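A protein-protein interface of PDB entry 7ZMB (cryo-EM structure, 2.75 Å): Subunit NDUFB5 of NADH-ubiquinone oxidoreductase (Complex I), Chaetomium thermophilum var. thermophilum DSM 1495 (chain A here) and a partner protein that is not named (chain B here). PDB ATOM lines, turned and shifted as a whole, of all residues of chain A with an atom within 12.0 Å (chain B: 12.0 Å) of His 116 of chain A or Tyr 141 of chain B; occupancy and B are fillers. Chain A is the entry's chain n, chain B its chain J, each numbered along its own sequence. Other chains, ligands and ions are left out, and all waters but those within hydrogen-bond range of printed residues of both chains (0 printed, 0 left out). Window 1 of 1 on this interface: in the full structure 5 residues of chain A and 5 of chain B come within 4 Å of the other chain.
A ring nitrogen (NE2) of His 116 of chain A is in hydrogen-bond range of the backbone carbonyl oxygen (O) of Tyr 141 of chain B.
The side-chain carboxylate (OE2) of Glu 145 of chain B is in salt-bridge range of the side-chain amino group (NZ) of Lys 149 of chain B (3.8 Å).
The backbone NH (N) of Tyr 141 of chain B lies within hydrogen-bond range of the side-chain carboxylate (OD1) of Asp 139 of chain B, at 3.0 Å.
The side-chain hydroxyl (OG1) of Thr 120 of chain A lies within hydrogen-bond range of the backbone carbonyl oxygen (O) of His 116 of chain A, at 2.6 Å.
Printed residues of chain A that touch a printed residue of chain B: Ala 112, His 113, His 116, Leu 117 and Thr 120.
Hydrophobic or aromatic side chains of chain A that line the printed part of chain B: His 113, His 116 and Leu 117.
Along chain A the printed residues that touch a printed residue of chain B span positions 112 to 120.
Of the 17 printed residues of chain B, 5 touch a printed residue of chain A.
Printed residues of chain B that touch a printed residue of chain A: Glu 140, Tyr 141, Lys 144, Glu 145 and Arg 148.
Hydrophobic or aromatic side chains of chain B within 4 Å of the printed part of chain A: Tyr 141.
Among the printed residues, 9 pairs touch across the chains.
Among the printed residues, no Asp or Glu carboxylate lies within 4 Å of a Lys or Arg side-chain nitrogen of the other chain.
Glu 109 of chain A touches none of the printed residues of chain B.
His 113 of chain A touches one residue of chain B.
No residue of chain B comes within 4 Å of Asp 114 of chain A.
No residue of chain B comes within 4 Å of Lys 115 of chain A.
His 116 of chain A touches just these residues of chain B: Tyr 141 (2.6 Å), Lys 144 (3.5 Å), Glu 145 (3.7 Å) and Arg 148 (3.4 Å).
Leu 117 of chain A touches one residue of chain B.
No residue of chain B comes within 4 Å of Leu 118 of chain A.
No residue of chain B comes within 4 Å of Leu 119 of chain A.
Of chain B, only Glu 140 and Tyr 141 come within 4 Å of Thr 120 of chain A.
Asp 139 of chain B touches none of the printed residues of chain A.
Glu 140 of chain B touches just one residue of chain A: Thr 120 (3.9 Å).
Tyr 141 of chain B touches just these residues of chain A: His 113 (3.2 Å), His 116 (2.6 Å), Leu 117 (3.3 Å) and Thr 120 (3.4 Å).
No residue of chain A comes within 4 Å of Glu 142 of chain B.
Lys 144 of chain B touches just one residue of chain A: His 116.
Of the printed residues of chain A, Glu 145 of chain B touches His 116 (3.7 Å).
Printed residues of chain A within 4 Å of Arg 148 of chain B: Ala 112 (3.6 Å) and His 116 (3.4 Å).
The nearest residue of chain A that does not touch Tyr 141 of chain B is Ala 121 of chain A (6.2 Å).
Ala 112 of chain A touches Arg 148 of chain B.
His 113 of chain A touches Tyr 141 of chain B.
CB of Lys 144 of chain B touches NE2 of His 116 of chain A, at 3.5 Å.
CE1 of His 116 of chain A touches CB of Glu 145 of chain B (3.7 Å).
Arg 148 of chain B touches His 116 of chain A.
Tyr 141 of chain B touches Leu 117 of chain A.
Thr 120 of chain A touches Glu 140 of chain B (CG2 to O, 3.9 Å).
Thr 120 of chain A touches Tyr 141 of chain B.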
ATOM      1  N   ALA A 107     -34.642  -3.195  12.374  1.00  0.00           N
ATOM      2  CA  ALA A 107     -33.942  -4.379  11.897  1.00  0.00           C
ATOM      3  C   ALA A 107     -33.061  -4.066  10.697  1.00  0.00           C
ATOM      4  O   ALA A 107     -31.993  -4.667  10.543  1.00  0.00           O
ATOM      5  CB  ALA A 107     -34.951  -5.474  11.549  1.00  0.00           C
ATOM      6  N   LEU A 108     -33.485  -3.137   9.843  1.00  0.00           N
ATOM      7  CA  LEU A 108     -32.706  -2.756   8.672  1.00  0.00           C
ATOM      8  C   LEU A 108     -31.708  -1.643   8.961  1.00  0.00           C
ATOM      9  O   LEU A 108     -30.677  -1.569   8.290  1.00  0.00           O
ATOM     10  CB  LEU A 108     -33.643  -2.338   7.541  1.00  0.00           C
ATOM     11  CG  LEU A 108     -34.621  -3.432   7.131  1.00  0.00           C
ATOM     12  CD1 LEU A 108     -35.847  -2.813   6.556  1.00  0.00           C
ATOM     13  CD2 LEU A 108     -34.002  -4.365   6.129  1.00  0.00           C
ATOM     14  N   GLU A 109     -31.989  -0.770   9.933  1.00  0.00           N
ATOM     15  CA  GLU A 109     -30.938   0.082  10.478  1.00  0.00           C
ATOM     16  C   GLU A 109     -29.751  -0.762  10.921  1.00  0.00           C
ATOM     17  O   GLU A 109     -28.604  -0.505  10.540  1.00  0.00           O
ATOM     18  CB  GLU A 109     -31.450   0.884  11.673  1.00  0.00           C
ATOM     19  CG  GLU A 109     -32.514   1.938  11.446  1.00  0.00           C
ATOM     20  CD  GLU A 109     -32.034   3.111  10.626  1.00  0.00           C
ATOM     21  OE1 GLU A 109     -30.837   3.455  10.705  1.00  0.00           O
ATOM     22  OE2 GLU A 109     -32.878   3.738   9.964  1.00  0.00           O
ATOM     23  N   GLN A 110     -30.020  -1.783  11.736  1.00  0.00           N
ATOM     24  CA  GLN A 110     -28.940  -2.599  12.271  1.00  0.00           C
ATOM     25  C   GLN A 110     -28.216  -3.345  11.161  1.00  0.00           C
ATOM     26  O   GLN A 110     -26.981  -3.403  11.147  1.00  0.00           O
ATOM     27  CB  GLN A 110     -29.480  -3.571  13.317  1.00  0.00           C
ATOM     28  CG  GLN A 110     -28.402  -4.164  14.199  1.00  0.00           C
ATOM     29  CD  GLN A 110     -27.459  -3.111  14.747  1.00  0.00           C
ATOM     30  OE1 GLN A 110     -26.388  -2.868  14.190  1.00  0.00           O
ATOM     31  NE2 GLN A 110     -27.854  -2.479  15.847  1.00  0.00           N
ATOM     32  N   ALA A 111     -28.966  -3.893  10.205  1.00  0.00           N
ATOM     33  CA  ALA A 111     -28.341  -4.555   9.069  1.00  0.00           C
ATOM     34  C   ALA A 111     -27.485  -3.586   8.270  1.00  0.00           C
ATOM     35  O   ALA A 111     -26.385  -3.935   7.834  1.00  0.00           O
ATOM     36  CB  ALA A 111     -29.406  -5.191   8.178  1.00  0.00           C
ATOM     37  N   ALA A 112     -27.970  -2.358   8.078  1.00  0.00           N
ATOM     38  CA  ALA A 112     -27.201  -1.366   7.333  1.00  0.00           C
ATOM     39  C   ALA A 112     -25.890  -1.044   8.035  1.00  0.00           C
ATOM     40  O   ALA A 112     -24.867  -0.818   7.382  1.00  0.00           O
ATOM     41  CB  ALA A 112     -28.028  -0.098   7.136  1.00  0.00           C
ATOM     42  N   HIS A 113     -25.909  -1.028   9.366  1.00  0.00           N
ATOM     43  CA  HIS A 113     -24.676  -0.760  10.150  1.00  0.00           C
ATOM     44  C   HIS A 113     -23.712  -1.939  10.011  1.00  0.00           C
ATOM     45  O   HIS A 113     -22.503  -1.699   9.908  1.00  0.00           O
ATOM     46  CB  HIS A 113     -25.020  -0.489  11.617  1.00  0.00           C
ATOM     47  CG  HIS A 113     -23.836  -0.540  12.522  1.00  0.00           C
ATOM     48  ND1 HIS A 113     -22.872   0.449  12.531  1.00  0.00           N
ATOM     49  CD2 HIS A 113     -23.450  -1.456  13.435  1.00  0.00           C
ATOM     50  CE1 HIS A 113     -21.944   0.145  13.415  1.00  0.00           C
ATOM     51  NE2 HIS A 113     -22.276  -1.019  13.983  1.00  0.00           N
ATOM     52  N   ASP A 114     -24.239  -3.163  10.035  1.00  0.00           N
ATOM     53  CA  ASP A 114     -23.376  -4.333   9.908  1.00  0.00           C
ATOM     54  C   ASP A 114     -22.669  -4.343   8.565  1.00  0.00           C
ATOM     55  O   ASP A 114     -21.461  -4.584   8.487  1.00  0.00           O
ATOM     56  CB  ASP A 114     -24.188  -5.614  10.097  1.00  0.00           C
ATOM     57  CG  ASP A 114     -25.004  -5.604  11.373  1.00  0.00           C
ATOM     58  OD1 ASP A 114     -24.582  -4.946  12.346  1.00  0.00           O
ATOM     59  OD2 ASP A 114     -26.070  -6.254  11.401  1.00  0.00           O
ATOM     60  N   LYS A 115     -23.412  -4.067   7.491  1.00  0.00           N
ATOM     61  CA  LYS A 115     -22.802  -3.983   6.171  1.00  0.00           C
ATOM     62  C   LYS A 115     -21.779  -2.864   6.124  1.00  0.00           C
ATOM     63  O   LYS A 115     -20.699  -3.024   5.547  1.00  0.00           O
ATOM     64  CB  LYS A 115     -23.886  -3.784   5.112  1.00  0.00           C
ATOM     65  CG  LYS A 115     -23.375  -3.424   3.725  1.00  0.00           C
ATOM     66  CD  LYS A 115     -24.524  -3.316   2.731  1.00  0.00           C
ATOM     67  CE  LYS A 115     -24.155  -2.456   1.530  1.00  0.00           C
ATOM     68  NZ  LYS A 115     -24.433  -1.007   1.759  1.00  0.00           N
ATOM     69  N   HIS A 116     -22.090  -1.731   6.753  1.00  0.00           N
ATOM     70  CA  HIS A 116     -21.146  -0.619   6.810  1.00  0.00           C
ATOM     71  C   HIS A 116     -19.860  -1.025   7.520  1.00  0.00           C
ATOM     72  O   HIS A 116     -18.763  -0.664   7.087  1.00  0.00           O
ATOM     73  CB  HIS A 116     -21.820   0.569   7.490  1.00  0.00           C
ATOM     74  CG  HIS A 116     -20.880   1.634   7.955  1.00  0.00           C
ATOM     75  ND1 HIS A 116     -20.972   2.207   9.205  1.00  0.00           N
ATOM     76  CD2 HIS A 116     -19.845   2.246   7.336  1.00  0.00           C
ATOM     77  CE1 HIS A 116     -20.031   3.120   9.338  1.00  0.00           C
ATOM     78  NE2 HIS A 116     -19.331   3.162   8.219  1.00  0.00           N
ATOM     79  N   LEU A 117     -19.979  -1.800   8.598  1.00  0.00           N
ATOM     80  CA  LEU A 117     -18.810  -2.351   9.274  1.00  0.00           C
ATOM     81  C   LEU A 117     -18.002  -3.273   8.367  1.00  0.00           C
ATOM     82  O   LEU A 117     -16.769  -3.199   8.335  1.00  0.00           O
ATOM     83  CB  LEU A 117     -19.263  -3.112  10.518  1.00  0.00           C
ATOM     84  CG  LEU A 117     -18.416  -3.174  11.786  1.00  0.00           C
ATOM     85  CD1 LEU A 117     -18.084  -1.815  12.302  1.00  0.00           C
ATOM     86  CD2 LEU A 117     -19.162  -3.970  12.837  1.00  0.00           C
ATOM     87  N   LEU A 118     -18.651  -4.279   7.789  1.00  0.00           N
ATOM     88  CA  LEU A 118     -17.932  -5.294   6.980  1.00  0.00           C
ATOM     89  C   LEU A 118     -17.318  -4.673   5.716  1.00  0.00           C
ATOM     90  O   LEU A 118     -16.170  -5.020   5.398  1.00  0.00           O
ATOM     91  CB  LEU A 118     -18.891  -6.447   6.668  1.00  0.00           C
ATOM     92  CG  LEU A 118     -19.372  -7.270   7.860  1.00  0.00           C
ATOM     93  CD1 LEU A 118     -20.724  -7.895   7.564  1.00  0.00           C
ATOM     94  CD2 LEU A 118     -18.361  -8.343   8.224  1.00  0.00           C
ATOM     95  N   LEU A 119     -18.058  -3.841   4.991  1.00  0.00           N
ATOM     96  CA  LEU A 119     -17.542  -3.215   3.740  1.00  0.00           C
ATOM     97  C   LEU A 119     -16.367  -2.274   4.018  1.00  0.00           C
ATOM     98  O   LEU A 119     -15.461  -2.221   3.179  1.00  0.00           O
ATOM     99  CB  LEU A 119     -18.669  -2.501   2.993  1.00  0.00           C
ATOM    100  CG  LEU A 119     -19.017  -3.095   1.630  1.00  0.00           C
ATOM    101  CD1 LEU A 119     -19.535  -4.516   1.780  1.00  0.00           C
ATOM    102  CD2 LEU A 119     -20.037  -2.230   0.908  1.00  0.00           C
ATOM    103  N   THR A 120     -16.397  -1.529   5.123  1.00  0.00           N
ATOM    104  CA  THR A 120     -15.344  -0.512   5.366  1.00  0.00           C
ATOM    105  C   THR A 120     -14.235  -1.047   6.267  1.00  0.00           C
ATOM    106  O   THR A 120     -13.488  -0.214   6.798  1.00  0.00           O
ATOM    107  CB  THR A 120     -15.930   0.764   5.973  1.00  0.00           C
ATOM    108  OG1 THR A 120     -16.403   0.435   7.278  1.00  0.00           O
ATOM    109  CG2 THR A 120     -17.039   1.367   5.139  1.00  0.00           C
ATOM    110  N   ALA A 121     -14.106  -2.368   6.404  1.00  0.00           N
ATOM    111  CA  ALA A 121     -13.047  -2.975   7.241  1.00  0.00           C
ATOM    112  C   ALA A 121     -11.680  -2.715   6.617  1.00  0.00           C
ATOM    113  O   ALA A 121     -11.554  -2.830   5.394  1.00  0.00           O
ATOM    114  CB  ALA A 121     -13.294  -4.443   7.393  1.00  0.00           C
ATOM    115  N   GLU A 122     -10.687  -2.396   7.442  1.00  0.00           N
ATOM    116  CA  GLU A 122      -9.338  -2.046   6.923  1.00  0.00           C
ATOM    117  C   GLU A 122      -8.681  -3.236   6.225  1.00  0.00           C
ATOM    118  O   GLU A 122      -8.829  -4.367   6.718  1.00  0.00           O
ATOM    119  CB  GLU A 122      -8.450  -1.567   8.069  1.00  0.00           C
ATOM    120  CG  GLU A 122      -9.040  -0.396   8.833  1.00  0.00           C
ATOM    121  CD  GLU A 122      -8.133   0.190   9.901  1.00  0.00           C
ATOM    122  OE1 GLU A 122      -8.652   0.874  10.805  1.00  0.00           O
ATOM    123  OE2 GLU A 122      -6.909  -0.038   9.824  1.00  0.00           O
ATOM    124  N   ARG A 123      -7.988  -2.980   5.116  1.00  0.00           N
ATOM    125  CA  ARG A 123      -7.211  -4.046   4.435  1.00  0.00           C
ATOM    126  C   ARG A 123      -5.900  -4.154   5.201  1.00  0.00           C
ATOM    127  O   ARG A 123      -5.348  -3.097   5.560  1.00  0.00           O
ATOM    128  CB  ARG A 123      -6.894  -3.605   3.004  1.00  0.00           C
ATOM    129  CG  ARG A 123      -6.051  -4.555   2.173  1.00  0.00           C
ATOM    130  CD  ARG A 123      -5.628  -3.776   0.945  1.00  0.00           C
ATOM    131  NE  ARG A 123      -5.239  -4.596  -0.189  1.00  0.00           N
ATOM    132  CZ  ARG A 123      -5.938  -4.686  -1.310  1.00  0.00           C
ATOM    133  NH1 ARG A 123      -7.055  -3.996  -1.450  1.00  0.00           N
ATOM    134  NH2 ARG A 123      -5.511  -5.456  -2.291  1.00  0.00           N
ATOM    135  N   LYS B 135      -6.554   8.300  -3.076  1.00  0.00           N
ATOM    136  CA  LYS B 135      -6.434   7.516  -1.855  1.00  0.00           C
ATOM    137  C   LYS B 135      -7.287   8.121  -0.749  1.00  0.00           C
ATOM    138  O   LYS B 135      -7.357   9.345  -0.595  1.00  0.00           O
ATOM    139  CB  LYS B 135      -4.973   7.443  -1.412  1.00  0.00           C
ATOM    140  N   ARG B 136      -7.947   7.255   0.021  1.00  0.00           N
ATOM    141  CA  ARG B 136      -8.810   7.730   1.097  1.00  0.00           C
ATOM    142  C   ARG B 136      -8.006   8.446   2.176  1.00  0.00           C
ATOM    143  O   ARG B 136      -8.327   9.579   2.556  1.00  0.00           O
ATOM    144  CB  ARG B 136      -9.593   6.560   1.695  1.00  0.00           C
ATOM    145  N   ASP B 137      -6.958   7.793   2.687  1.00  0.00           N
ATOM    146  CA  ASP B 137      -6.091   8.342   3.727  1.00  0.00           C
ATOM    147  C   ASP B 137      -6.866   8.720   4.986  1.00  0.00           C
ATOM    148  O   ASP B 137      -6.335   9.414   5.859  1.00  0.00           O
ATOM    149  CB  ASP B 137      -5.326   9.561   3.201  1.00  0.00           C
ATOM    150  CG  ASP B 137      -4.493   9.242   1.977  1.00  0.00           C
ATOM    151  OD1 ASP B 137      -4.068   8.077   1.834  1.00  0.00           O
ATOM    152  OD2 ASP B 137      -4.263  10.155   1.158  1.00  0.00           O
ATOM    153  N   VAL B 138      -8.117   8.268   5.093  1.00  0.00           N
ATOM    154  CA  VAL B 138      -8.985   8.597   6.216  1.00  0.00           C
ATOM    155  C   VAL B 138      -9.781   7.359   6.602  1.00  0.00           C
ATOM    156  O   VAL B 138      -9.766   6.338   5.911  1.00  0.00           O
ATOM    157  CB  VAL B 138      -9.951   9.763   5.903  1.00  0.00           C
ATOM    158  CG1 VAL B 138      -9.184  11.058   5.677  1.00  0.00           C
ATOM    159  CG2 VAL B 138     -10.810   9.425   4.695  1.00  0.00           C
ATOM    160  N   ASP B 139     -10.486   7.465   7.725  1.00  0.00           N
ATOM    161  CA  ASP B 139     -11.342   6.383   8.193  1.00  0.00           C
ATOM    162  C   ASP B 139     -12.536   6.249   7.259  1.00  0.00           C
ATOM    163  O   ASP B 139     -13.425   7.106   7.246  1.00  0.00           O
ATOM    164  CB  ASP B 139     -11.791   6.647   9.626  1.00  0.00           C
ATOM    165  CG  ASP B 139     -12.290   5.393  10.322  1.00  0.00           C
ATOM    166  OD1 ASP B 139     -12.743   4.464   9.624  1.00  0.00           O
ATOM    167  OD2 ASP B 139     -12.229   5.338  11.568  1.00  0.00           O
ATOM    168  N   GLU B 140     -12.554   5.176   6.467  1.00  0.00           N
ATOM    169  CA  GLU B 140     -13.690   4.930   5.591  1.00  0.00           C
ATOM    170  C   GLU B 140     -14.945   4.619   6.388  1.00  0.00           C
ATOM    171  O   GLU B 140     -16.047   4.997   5.977  1.00  0.00           O
ATOM    172  CB  GLU B 140     -13.373   3.786   4.627  1.00  0.00           C
ATOM    173  N   TYR B 141     -14.800   3.932   7.522  1.00  0.00           N
ATOM    174  CA  TYR B 141     -15.951   3.688   8.383  1.00  0.00           C
ATOM    175  C   TYR B 141     -16.556   5.000   8.861  1.00  0.00           C
ATOM    176  O   TYR B 141     -17.781   5.162   8.866  1.00  0.00           O
ATOM    177  CB  TYR B 141     -15.542   2.804   9.563  1.00  0.00           C
ATOM    178  CG  TYR B 141     -16.605   2.646  10.625  1.00  0.00           C
ATOM    179  CD1 TYR B 141     -16.759   3.592  11.631  1.00  0.00           C
ATOM    180  CD2 TYR B 141     -17.453   1.549  10.630  1.00  0.00           C
ATOM    181  CE1 TYR B 141     -17.722   3.462  12.586  1.00  0.00           C
ATOM    182  CE2 TYR B 141     -18.424   1.413  11.595  1.00  0.00           C
ATOM    183  CZ  TYR B 141     -18.553   2.372  12.569  1.00  0.00           C
ATOM    184  OH  TYR B 141     -19.518   2.250  13.545  1.00  0.00           O
ATOM    185  N   GLU B 142     -15.710   5.949   9.264  1.00  0.00           N
ATOM    186  CA  GLU B 142     -16.206   7.227   9.763  1.00  0.00           C
ATOM    187  C   GLU B 142     -16.874   8.039   8.661  1.00  0.00           C
ATOM    188  O   GLU B 142     -17.929   8.643   8.885  1.00  0.00           O
ATOM    189  CB  GLU B 142     -15.061   8.022  10.391  1.00  0.00           C
ATOM    190  CG  GLU B 142     -15.489   9.340  11.012  1.00  0.00           C
ATOM    191  CD  GLU B 142     -14.339  10.080  11.670  1.00  0.00           C
ATOM    192  OE1 GLU B 142     -13.198   9.571  11.624  1.00  0.00           O
ATOM    193  OE2 GLU B 142     -14.575  11.171  12.230  1.00  0.00           O
ATOM    194  N   ARG B 143     -16.278   8.070   7.468  1.00  0.00           N
ATOM    195  CA  ARG B 143     -16.829   8.882   6.389  1.00  0.00           C
ATOM    196  C   ARG B 143     -18.235   8.431   6.024  1.00  0.00           C
ATOM    197  O   ARG B 143     -19.123   9.259   5.799  1.00  0.00           O
ATOM    198  CB  ARG B 143     -15.914   8.830   5.168  1.00  0.00           C
ATOM    199  CG  ARG B 143     -16.371   9.700   4.007  1.00  0.00           C
ATOM    200  CD  ARG B 143     -15.405   9.603   2.834  1.00  0.00           C
ATOM    201  NE  ARG B 143     -15.340   8.252   2.287  1.00  0.00           N
ATOM    202  CZ  ARG B 143     -16.206   7.758   1.408  1.00  0.00           C
ATOM    203  NH1 ARG B 143     -17.201   8.512   0.960  1.00  0.00           N
ATOM    204  NH2 ARG B 143     -16.071   6.516   0.967  1.00  0.00           N
ATOM    205  N   LYS B 144     -18.454   7.122   5.957  1.00  0.00           N
ATOM    206  CA  LYS B 144     -19.791   6.613   5.688  1.00  0.00           C
ATOM    207  C   LYS B 144     -20.725   6.885   6.852  1.00  0.00           C
ATOM    208  O   LYS B 144     -21.901   7.207   6.651  1.00  0.00           O
ATOM    209  CB  LYS B 144     -19.721   5.120   5.386  1.00  0.00           C
ATOM    210  CG  LYS B 144     -18.910   4.792   4.154  1.00  0.00           C
ATOM    211  CD  LYS B 144     -19.493   5.458   2.932  1.00  0.00           C
ATOM    212  CE  LYS B 144     -19.214   4.648   1.680  1.00  0.00           C
ATOM    213  NZ  LYS B 144     -19.974   3.374   1.671  1.00  0.00           N
ATOM    214  N   GLU B 145     -20.221   6.755   8.079  1.00  0.00           N
ATOM    215  CA  GLU B 145     -21.043   7.019   9.254  1.00  0.00           C
ATOM    216  C   GLU B 145     -21.436   8.488   9.334  1.00  0.00           C
ATOM    217  O   GLU B 145     -22.558   8.818   9.737  1.00  0.00           O
ATOM    218  CB  GLU B 145     -20.297   6.576  10.512  1.00  0.00           C
ATOM    219  CG  GLU B 145     -21.113   6.605  11.780  1.00  0.00           C
ATOM    220  CD  GLU B 145     -21.031   7.942  12.494  1.00  0.00           C
ATOM    221  OE1 GLU B 145     -20.066   8.695  12.241  1.00  0.00           O
ATOM    222  OE2 GLU B 145     -21.928   8.238  13.308  1.00  0.00           O
ATOM    223  N   PHE B 146     -20.530   9.390   8.947  1.00  0.00           N
ATOM    224  CA  PHE B 146     -20.841  10.814   9.031  1.00  0.00           C
ATOM    225  C   PHE B 146     -21.854  11.228   7.973  1.00  0.00           C
ATOM    226  O   PHE B 146     -22.812  11.948   8.277  1.00  0.00           O
ATOM    227  CB  PHE B 146     -19.564  11.644   8.912  1.00  0.00           C
ATOM    228  CG  PHE B 146     -19.815  13.121   8.773  1.00  0.00           C
ATOM    229  CD1 PHE B 146     -20.686  13.774   9.632  1.00  0.00           C
ATOM    230  CD2 PHE B 146     -19.179  13.855   7.787  1.00  0.00           C
ATOM    231  CE1 PHE B 146     -20.923  15.122   9.506  1.00  0.00           C
ATOM    232  CE2 PHE B 146     -19.410  15.210   7.658  1.00  0.00           C
ATOM    233  CZ  PHE B 146     -20.283  15.844   8.519  1.00  0.00           C
ATOM    234  N   LEU B 147     -21.673  10.774   6.729  1.00  0.00           N
ATOM    235  CA  LEU B 147     -22.596  11.119   5.651  1.00  0.00           C
ATOM    236  C   LEU B 147     -23.988  10.548   5.840  1.00  0.00           C
ATOM    237  O   LEU B 147     -24.910  10.969   5.135  1.00  0.00           O
ATOM    238  CB  LEU B 147     -22.060  10.645   4.305  1.00  0.00           C
ATOM    239  CG  LEU B 147     -20.803  11.282   3.757  1.00  0.00           C
ATOM    240  CD1 LEU B 147     -20.394  10.567   2.507  1.00  0.00           C
ATOM    241  CD2 LEU B 147     -21.098  12.724   3.459  1.00  0.00           C
ATOM    242  N   ARG B 148     -24.161   9.610   6.759  1.00  0.00           N
ATOM    243  CA  ARG B 148     -25.422   8.921   6.952  1.00  0.00           C
ATOM    244  C   ARG B 148     -26.222   9.454   8.128  1.00  0.00           C
ATOM    245  O   ARG B 148     -27.453   9.372   8.115  1.00  0.00           O
ATOM    246  CB  ARG B 148     -25.144   7.433   7.155  1.00  0.00           C
ATOM    247  CG  ARG B 148     -26.338   6.534   7.295  1.00  0.00           C
ATOM    248  CD  ARG B 148     -25.804   5.146   7.501  1.00  0.00           C
ATOM    249  NE  ARG B 148     -24.721   4.901   6.552  1.00  0.00           N
ATOM    250  CZ  ARG B 148     -24.075   3.751   6.420  1.00  0.00           C
ATOM    251  NH1 ARG B 148     -23.106   3.641   5.524  1.00  0.00           N
ATOM    252  NH2 ARG B 148     -24.403   2.713   7.173  1.00  0.00           N
ATOM    253  N   LYS B 149     -25.557  10.002   9.140  1.00  0.00           N
ATOM    254  CA  LYS B 149     -26.220  10.435  10.359  1.00  0.00           C
ATOM    255  C   LYS B 149     -26.173  11.943  10.548  1.00  0.00           C
ATOM    256  O   LYS B 149     -26.564  12.437  11.612  1.00  0.00           O
ATOM    257  CB  LYS B 149     -25.610   9.726  11.568  1.00  0.00           C
ATOM    258  CG  LYS B 149     -25.847   8.231  11.571  1.00  0.00           C
ATOM    259  CD  LYS B 149     -26.084   7.697  12.975  1.00  0.00           C
ATOM    260  CE  LYS B 149     -25.033   8.188  13.955  1.00  0.00           C
ATOM    261  NZ  LYS B 149     -25.049   7.411  15.223  1.00  0.00           N
ATOM    262  N   ASN B 150     -25.711  12.691   9.547  1.00  0.00           N
ATOM    263  CA  ASN B 150     -25.820  14.150   9.563  1.00  0.00           C
ATOM    264  C   ASN B 150     -27.196  14.543   9.015  1.00  0.00           C
ATOM    265  O   ASN B 150     -27.335  15.223   7.998  1.00  0.00           O
ATOM    266  CB  ASN B 150     -24.690  14.779   8.762  1.00  0.00           C
ATOM    267  CG  ASN B 150     -24.529  16.256   9.046  1.00  0.00           C
ATOM    268  OD1 ASN B 150     -25.302  16.842   9.801  1.00  0.00           O
ATOM    269  ND2 ASN B 150     -23.517  16.867   8.443  1.00  0.00           N
ATOM    270  N   ARG B 151     -28.231  14.092   9.725  1.00  0.00           N
ATOM    271  CA  ARG B 151     -29.603  14.211   9.245  1.00  0.00           C
ATOM    272  C   ARG B 151     -30.176  15.616   9.379  1.00  0.00           C
ATOM    273  O   ARG B 151     -31.028  16.002   8.572  1.00  0.00           O
ATOM    274  CB  ARG B 151     -30.504  13.217   9.981  1.00  0.00           C
ATOM    275  CG  ARG B 151     -30.193  11.776   9.641  1.00  0.00           C
ATOM    276  CD  ARG B 151     -31.096  10.812  10.379  1.00  0.00           C
ATOM    277  NE  ARG B 151     -30.793   9.436  10.022  1.00  0.00           N
ATOM    278  CZ  ARG B 151     -29.916   8.684  10.678  1.00  0.00           C
ATOM    279  NH1 ARG B 151     -29.681   7.438  10.292  1.00  0.00           N
ATOM    280  NH2 ARG B 151     -29.273   9.179  11.724  1.00  0.00           N
